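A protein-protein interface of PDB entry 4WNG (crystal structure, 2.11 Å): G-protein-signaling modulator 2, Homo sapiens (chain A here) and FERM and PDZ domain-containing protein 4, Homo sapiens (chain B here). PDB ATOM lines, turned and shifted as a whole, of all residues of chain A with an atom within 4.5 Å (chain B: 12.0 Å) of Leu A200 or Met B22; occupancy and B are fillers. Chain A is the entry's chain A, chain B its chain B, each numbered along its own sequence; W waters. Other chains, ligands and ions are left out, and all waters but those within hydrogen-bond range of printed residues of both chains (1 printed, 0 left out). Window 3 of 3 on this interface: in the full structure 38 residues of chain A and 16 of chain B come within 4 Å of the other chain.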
ATOM      1  N   HIS A 139      14.943  10.074   8.151  1.00  0.00           N
ATOM      2  CA  HIS A 139      15.724   9.555   9.273  1.00  0.00           C
ATOM      3  C   HIS A 139      16.115   8.105   9.050  1.00  0.00           C
ATOM      4  O   HIS A 139      17.268   7.751   9.222  1.00  0.00           O
ATOM      5  CB  HIS A 139      14.912   9.649  10.573  1.00  0.00           C
ATOM      6  CG  HIS A 139      15.556   8.955  11.735  1.00  0.00           C
ATOM      7  ND1 HIS A 139      16.251   9.634  12.703  1.00  0.00           N
ATOM      8  CD2 HIS A 139      15.620   7.644  12.077  1.00  0.00           C
ATOM      9  CE1 HIS A 139      16.734   8.779  13.587  1.00  0.00           C
ATOM     10  NE2 HIS A 139      16.355   7.564  13.236  1.00  0.00           N
ATOM     11  N   LYS A 143      19.881   6.740   8.393  1.00  0.00           N
ATOM     12  CA  LYS A 143      20.382   5.758   9.354  1.00  0.00           C
ATOM     13  C   LYS A 143      20.732   4.400   8.699  1.00  0.00           C
ATOM     14  O   LYS A 143      21.575   3.685   9.211  1.00  0.00           O
ATOM     15  CB  LYS A 143      19.346   5.568  10.469  1.00  0.00           C
ATOM     16  CG  LYS A 143      19.764   4.617  11.589  1.00  0.00           C
ATOM     17  CD  LYS A 143      18.779   4.642  12.756  1.00  0.00           C
ATOM     18  CE  LYS A 143      17.420   4.060  12.382  1.00  0.00           C
ATOM     19  NZ  LYS A 143      16.383   4.209  13.453  1.00  0.00           N
ATOM     20  N   PHE A 156      29.943  11.192   7.927  1.00  0.00           N
ATOM     21  CA  PHE A 156      28.908  10.753   6.978  1.00  0.00           C
ATOM     22  C   PHE A 156      29.112  11.253   5.564  1.00  0.00           C
ATOM     23  O   PHE A 156      29.520  12.391   5.367  1.00  0.00           O
ATOM     24  CB  PHE A 156      27.529  11.292   7.388  1.00  0.00           C
ATOM     25  CG  PHE A 156      26.942  10.638   8.589  1.00  0.00           C
ATOM     26  CD1 PHE A 156      26.817   9.258   8.660  1.00  0.00           C
ATOM     27  CD2 PHE A 156      26.466  11.408   9.641  1.00  0.00           C
ATOM     28  CE1 PHE A 156      26.264   8.657   9.777  1.00  0.00           C
ATOM     29  CE2 PHE A 156      25.911  10.813  10.755  1.00  0.00           C
ATOM     30  CZ  PHE A 156      25.808   9.436  10.825  1.00  0.00           C
ATOM     31  N   LEU A 164      19.477  13.270   6.944  1.00  0.00           N
ATOM     32  CA  LEU A 164      19.225  13.492   8.367  1.00  0.00           C
ATOM     33  C   LEU A 164      18.827  14.945   8.645  1.00  0.00           C
ATOM     34  O   LEU A 164      17.965  15.204   9.476  1.00  0.00           O
ATOM     35  CB  LEU A 164      20.448  13.096   9.186  1.00  0.00           C
ATOM     36  CG  LEU A 164      20.779  11.599   9.243  1.00  0.00           C
ATOM     37  CD1 LEU A 164      21.995  11.346  10.141  1.00  0.00           C
ATOM     38  CD2 LEU A 164      19.606  10.765   9.738  1.00  0.00           C
ATOM     39  N   ASN A 196      16.496  11.792  18.578  1.00  0.00           N
ATOM     40  CA  ASN A 196      17.266  10.705  17.934  1.00  0.00           C
ATOM     41  C   ASN A 196      17.990  11.149  16.681  1.00  0.00           C
ATOM     42  O   ASN A 196      19.138  10.716  16.417  1.00  0.00           O
ATOM     43  CB  ASN A 196      16.368   9.509  17.619  1.00  0.00           C
ATOM     44  CG  ASN A 196      15.782   8.888  18.869  1.00  0.00           C
ATOM     45  OD1 ASN A 196      16.339   9.034  19.948  1.00  0.00           O
ATOM     46  ND2 ASN A 196      14.654   8.220  18.736  1.00  0.00           N
ATOM     47  N   THR A 197      17.353  12.024  15.905  1.00  0.00           N
ATOM     48  CA  THR A 197      18.002  12.499  14.666  1.00  0.00           C
ATOM     49  C   THR A 197      19.185  13.396  15.002  1.00  0.00           C
ATOM     50  O   THR A 197      20.272  13.254  14.423  1.00  0.00           O
ATOM     51  CB  THR A 197      17.027  13.224  13.726  1.00  0.00           C
ATOM     52  OG1 THR A 197      15.904  12.379  13.466  1.00  0.00           O
ATOM     53  CG2 THR A 197      17.716  13.589  12.405  1.00  0.00           C
ATOM     54  N   HIS A 198      19.000  14.299  15.961  1.00  0.00           N
ATOM     55  CA  HIS A 198      20.133  15.100  16.457  1.00  0.00           C
ATOM     56  C   HIS A 198      21.262  14.217  17.007  1.00  0.00           C
ATOM     57  O   HIS A 198      22.447  14.487  16.805  1.00  0.00           O
ATOM     58  CB  HIS A 198      19.687  16.064  17.555  1.00  0.00           C
ATOM     59  CG  HIS A 198      18.965  17.265  17.049  1.00  0.00           C
ATOM     60  ND1 HIS A 198      19.476  18.078  16.067  1.00  0.00           N
ATOM     61  CD2 HIS A 198      17.805  17.831  17.439  1.00  0.00           C
ATOM     62  CE1 HIS A 198      18.647  19.080  15.850  1.00  0.00           C
ATOM     63  NE2 HIS A 198      17.619  18.945  16.661  1.00  0.00           N
ATOM     64  N   TYR A 199      20.891  13.190  17.749  1.00  0.00           N
ATOM     65  CA  TYR A 199      21.885  12.223  18.251  1.00  0.00           C
ATOM     66  C   TYR A 199      22.743  11.673  17.094  1.00  0.00           C
ATOM     67  O   TYR A 199      23.965  11.754  17.134  1.00  0.00           O
ATOM     68  CB  TYR A 199      21.173  11.100  18.992  1.00  0.00           C
ATOM     69  CG  TYR A 199      22.053  10.015  19.553  1.00  0.00           C
ATOM     70  CD1 TYR A 199      22.710  10.191  20.772  1.00  0.00           C
ATOM     71  CD2 TYR A 199      22.208   8.789  18.884  1.00  0.00           C
ATOM     72  CE1 TYR A 199      23.499   9.188  21.310  1.00  0.00           C
ATOM     73  CE2 TYR A 199      22.990   7.774  19.422  1.00  0.00           C
ATOM     74  CZ  TYR A 199      23.642   7.984  20.633  1.00  0.00           C
ATOM     75  OH  TYR A 199      24.442   7.003  21.187  1.00  0.00           O
ATOM     76  N   LEU A 200      22.098  11.174  16.047  1.00  0.00           N
ATOM     77  CA  LEU A 200      22.823  10.606  14.916  1.00  0.00           C
ATOM     78  C   LEU A 200      23.680  11.633  14.211  1.00  0.00           C
ATOM     79  O   LEU A 200      24.775  11.305  13.737  1.00  0.00           O
ATOM     80  CB  LEU A 200      21.863   9.978  13.906  1.00  0.00           C
ATOM     81  CG  LEU A 200      21.332   8.592  14.256  1.00  0.00           C
ATOM     82  CD1 LEU A 200      20.417   8.140  13.130  1.00  0.00           C
ATOM     83  CD2 LEU A 200      22.456   7.584  14.447  1.00  0.00           C
ATOM     84  N   LEU A 201      23.203  12.875  14.165  1.00  0.00           N
ATOM     85  CA  LEU A 201      24.003  13.968  13.625  1.00  0.00           C
ATOM     86  C   LEU A 201      25.135  14.441  14.539  1.00  0.00           C
ATOM     87  O   LEU A 201      25.885  15.326  14.161  1.00  0.00           O
ATOM     88  CB  LEU A 201      23.096  15.166  13.286  1.00  0.00           C
ATOM     89  CG  LEU A 201      22.223  14.990  12.054  1.00  0.00           C
ATOM     90  CD1 LEU A 201      21.100  16.029  12.020  1.00  0.00           C
ATOM     91  CD2 LEU A 201      23.103  15.089  10.809  1.00  0.00           C
ATOM     92  N   GLY A 202      25.239  13.907  15.751  1.00  0.00           N
ATOM     93  CA  GLY A 202      26.223  14.410  16.704  1.00  0.00           C
ATOM     94  C   GLY A 202      25.892  15.769  17.322  1.00  0.00           C
ATOM     95  O   GLY A 202      26.791  16.446  17.821  1.00  0.00           O
ATOM     96  N   ASN A 233      17.063   7.443  26.179  1.00  0.00           N
ATOM     97  CA  ASN A 233      17.661   8.291  25.130  1.00  0.00           C
ATOM     98  C   ASN A 233      18.492   9.427  25.738  1.00  0.00           C
ATOM     99  O   ASN A 233      19.556   9.786  25.215  1.00  0.00           O
ATOM    100  CB  ASN A 233      16.572   8.851  24.172  1.00  0.00           C
ATOM    101  CG  ASN A 233      15.990   7.778  23.241  1.00  0.00           C
ATOM    102  OD1 ASN A 233      16.712   6.933  22.753  1.00  0.00           O
ATOM    103  ND2 ASN A 233      14.675   7.808  23.012  1.00  0.00           N
ATOM    104  N   ASN A 236      21.918   8.025  26.827  1.00  0.00           N
ATOM    105  CA  ASN A 236      22.768   7.769  25.672  1.00  0.00           C
ATOM    106  C   ASN A 236      23.452   9.032  25.213  1.00  0.00           C
ATOM    107  O   ASN A 236      24.645   9.033  24.891  1.00  0.00           O
ATOM    108  CB  ASN A 236      21.942   7.212  24.491  1.00  0.00           C
ATOM    109  CG  ASN A 236      21.325   5.850  24.784  1.00  0.00           C
ATOM    110  OD1 ASN A 236      21.720   5.156  25.736  1.00  0.00           O
ATOM    111  ND2 ASN A 236      20.339   5.458  23.969  1.00  0.00           N
ATOM    112  N   HIS B  21      21.167   1.300  21.325  1.00  0.00           N
ATOM    113  CA  HIS B  21      20.366   1.944  20.241  1.00  0.00           C
ATOM    114  C   HIS B  21      19.384   2.998  20.754  1.00  0.00           C
ATOM    115  O   HIS B  21      18.729   2.826  21.790  1.00  0.00           O
ATOM    116  CB  HIS B  21      19.575   0.896  19.434  1.00  0.00           C
ATOM    117  CG  HIS B  21      20.290   0.416  18.210  1.00  0.00           C
ATOM    118  ND1 HIS B  21      20.302   1.128  17.030  1.00  0.00           N
ATOM    119  CD2 HIS B  21      21.024  -0.699  17.985  1.00  0.00           C
ATOM    120  CE1 HIS B  21      21.010   0.471  16.129  1.00  0.00           C
ATOM    121  NE2 HIS B  21      21.458  -0.641  16.683  1.00  0.00           N
ATOM    122  N   MET B  22      19.283   4.087  20.003  1.00  0.00           N
ATOM    123  CA  MET B  22      18.243   5.078  20.208  1.00  0.00           C
ATOM    124  C   MET B  22      16.897   4.386  20.023  1.00  0.00           C
ATOM    125  O   MET B  22      16.751   3.546  19.134  1.00  0.00           O
ATOM    126  CB  MET B  22      18.409   6.236  19.203  1.00  0.00           C
ATOM    127  CG  MET B  22      18.007   5.924  17.760  1.00  0.00           C
ATOM    128  SD  MET B  22      19.111   6.647  16.533  1.00  0.00           S
ATOM    129  CE  MET B  22      20.472   5.491  16.698  1.00  0.00           C
ATOM    130  N   GLU B  23      15.926   4.711  20.863  1.00  0.00           N
ATOM    131  CA  GLU B  23      14.611   4.113  20.741  1.00  0.00           C
ATOM    132  C   GLU B  23      13.661   5.112  20.130  1.00  0.00           C
ATOM    133  O   GLU B  23      13.524   6.243  20.614  1.00  0.00           O
ATOM    134  CB  GLU B  23      14.107   3.664  22.096  1.00  0.00           C
ATOM    135  CG  GLU B  23      15.146   2.841  22.840  1.00  0.00           C
ATOM    136  CD  GLU B  23      14.547   2.001  23.933  1.00  0.00           C
ATOM    137  OE1 GLU B  23      13.395   1.544  23.784  1.00  0.00           O
ATOM    138  OE2 GLU B  23      15.238   1.802  24.947  1.00  0.00           O
ATOM    139  N   MET B  24      13.000   4.670  19.070  1.00  0.00           N
ATOM    140  CA  MET B  24      12.196   5.526  18.235  1.00  0.00           C
ATOM    141  C   MET B  24      10.791   5.613  18.756  1.00  0.00           C
ATOM    142  O   MET B  24      10.316   4.704  19.428  1.00  0.00           O
ATOM    143  CB  MET B  24      12.178   4.961  16.813  1.00  0.00           C
ATOM    144  CG  MET B  24      13.573   4.832  16.206  1.00  0.00           C
ATOM    145  SD  MET B  24      14.389   6.434  15.965  1.00  0.00           S
ATOM    146  CE  MET B  24      13.349   7.057  14.646  1.00  0.00           C
ATOM    147  N   GLU B  25      10.120   6.712  18.442  1.00  0.00           N
ATOM    148  CA  GLU B  25       8.689   6.813  18.635  1.00  0.00           C
ATOM    149  C   GLU B  25       7.950   5.969  17.576  1.00  0.00           C
ATOM    150  O   GLU B  25       8.515   5.647  16.556  1.00  0.00           O
ATOM    151  CB  GLU B  25       8.256   8.283  18.569  1.00  0.00           C
ATOM    152  CG  GLU B  25       8.885   9.139  19.672  1.00  0.00           C
ATOM    153  CD  GLU B  25       8.500   8.635  21.053  1.00  0.00           C
ATOM    154  OE1 GLU B  25       7.309   8.345  21.254  1.00  0.00           O
ATOM    155  OE2 GLU B  25       9.391   8.464  21.910  1.00  0.00           O
ATOM    156  N   PRO B  26       6.685   5.600  17.833  1.00  0.00           N
ATOM    157  CA  PRO B  26       5.915   4.831  16.833  1.00  0.00           C
ATOM    158  C   PRO B  26       5.515   5.596  15.572  1.00  0.00           C
ATOM    159  O   PRO B  26       5.364   6.818  15.590  1.00  0.00           O
ATOM    160  CB  PRO B  26       4.648   4.419  17.600  1.00  0.00           C
ATOM    161  CG  PRO B  26       4.546   5.380  18.745  1.00  0.00           C
ATOM    162  CD  PRO B  26       5.976   5.685  19.123  1.00  0.00           C
ATOM    163  N   GLU B  27       5.321   4.864  14.477  1.00  0.00           N
ATOM    164  CA  GLU B  27       4.707   5.449  13.289  1.00  0.00           C
ATOM    165  C   GLU B  27       3.255   5.680  13.639  1.00  0.00           C
ATOM    166  O   GLU B  27       2.692   4.940  14.436  1.00  0.00           O
ATOM    167  CB  GLU B  27       4.767   4.512  12.085  1.00  0.00           C
ATOM    168  CG  GLU B  27       6.161   4.096  11.636  1.00  0.00           C
ATOM    169  CD  GLU B  27       6.669   2.815  12.278  1.00  0.00           C
ATOM    170  OE1 GLU B  27       5.921   2.154  13.043  1.00  0.00           O
ATOM    171  OE2 GLU B  27       7.838   2.477  12.024  1.00  0.00           O
HETATM  172  O   HOH W   1      11.872   8.723  21.416  1.00  0.00           O
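A ring nitrogen (NE2) of His A139 sits close to the side-chain sulfur (SD) of Met B24 (3.5 Å).
ND2 of Asn A196 is in hydrogen-bond range of O of Glu B23, at 3.0 Å.
The side-chain sulfur (SD) of Met B24 sits at hydrogen-bond distance from the side-chain amide nitrogen (ND2) of Asn A196, 3.3 Å away.
The side-chain amide oxygen (OD1) of Asn A233 is in hydrogen-bond range of the backbone NH (N) of Glu B23, 3.0 Å away.
NZ of Lys A143 sits at hydrogen-bond distance from NE2 of His A139 (3.4 Å).
The side-chain hydroxyl (OG1) of Thr A197 lies within hydrogen-bond range of a ring nitrogen (ND1) of His A139.
Among the printed residues, merely in contact across the chains: Asn A233 with Met B22, Asn A196 with Met B22, Leu A200 with Met B22, Asn A236 with His B21 and Lys A143 with Met B24.
Of the printed residues of chain B, Leu A200 touches Met B22 (3.7 Å).
Of chain B, only Met B24 comes within 4 Å of His A139.
Lys A143 touches just one residue of chain B: Met B24 (3.9 Å).
No residue of chain B comes within 4 Å of Thr A197.
No residue of chain B comes within 4 Å of Leu A201.
No residue of chain B comes within 4 Å of Gly A202.
Printed residues of chain B within 4 Å of Asn A236: His B21.
Of the printed residues of chain A, Met B24 touches His A139, Lys A143 and Asn A196.
Printed residues of chain B within 4 Å of Asn A233: Met B22 and Glu B23.
Printed residues of chain A within 4 Å of Glu B23: Asn A196 and Asn A233.
Phe A156 touches none of the printed residues of chain B.
Leu A164 touches none of the printed residues of chain B.
The nearest printed residue of chain A that does not touch Met B22 is Lys A143 (4.3 Å).
Printed residues of chain B that touch a printed residue of chain A: His B21, Met B22, Glu B23 and Met B24.
Hydrophobic or aromatic side chains of chain B that line the printed part of chain A: Met B22 and Met B24.
Of the 13 printed residues of chain A, 6 touch a printed residue of chain B.
Printed residues of chain A that touch a printed residue of chain B: His A139, Lys A143, Asn A196, Leu A200, Asn A233 and Asn A236.
Along chain A the printed residues that touch a printed residue of chain B span positions 139 to 236.
Water W1 lies within hydrogen-bond range of the side-chain carboxylate (OE2) of Glu B25 (2.5 Å), the backbone carbonyl oxygen (O) of Glu B23 (3.1 Å) and the side-chain amide nitrogen (ND2) of Asn A233 (3.4 Å).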
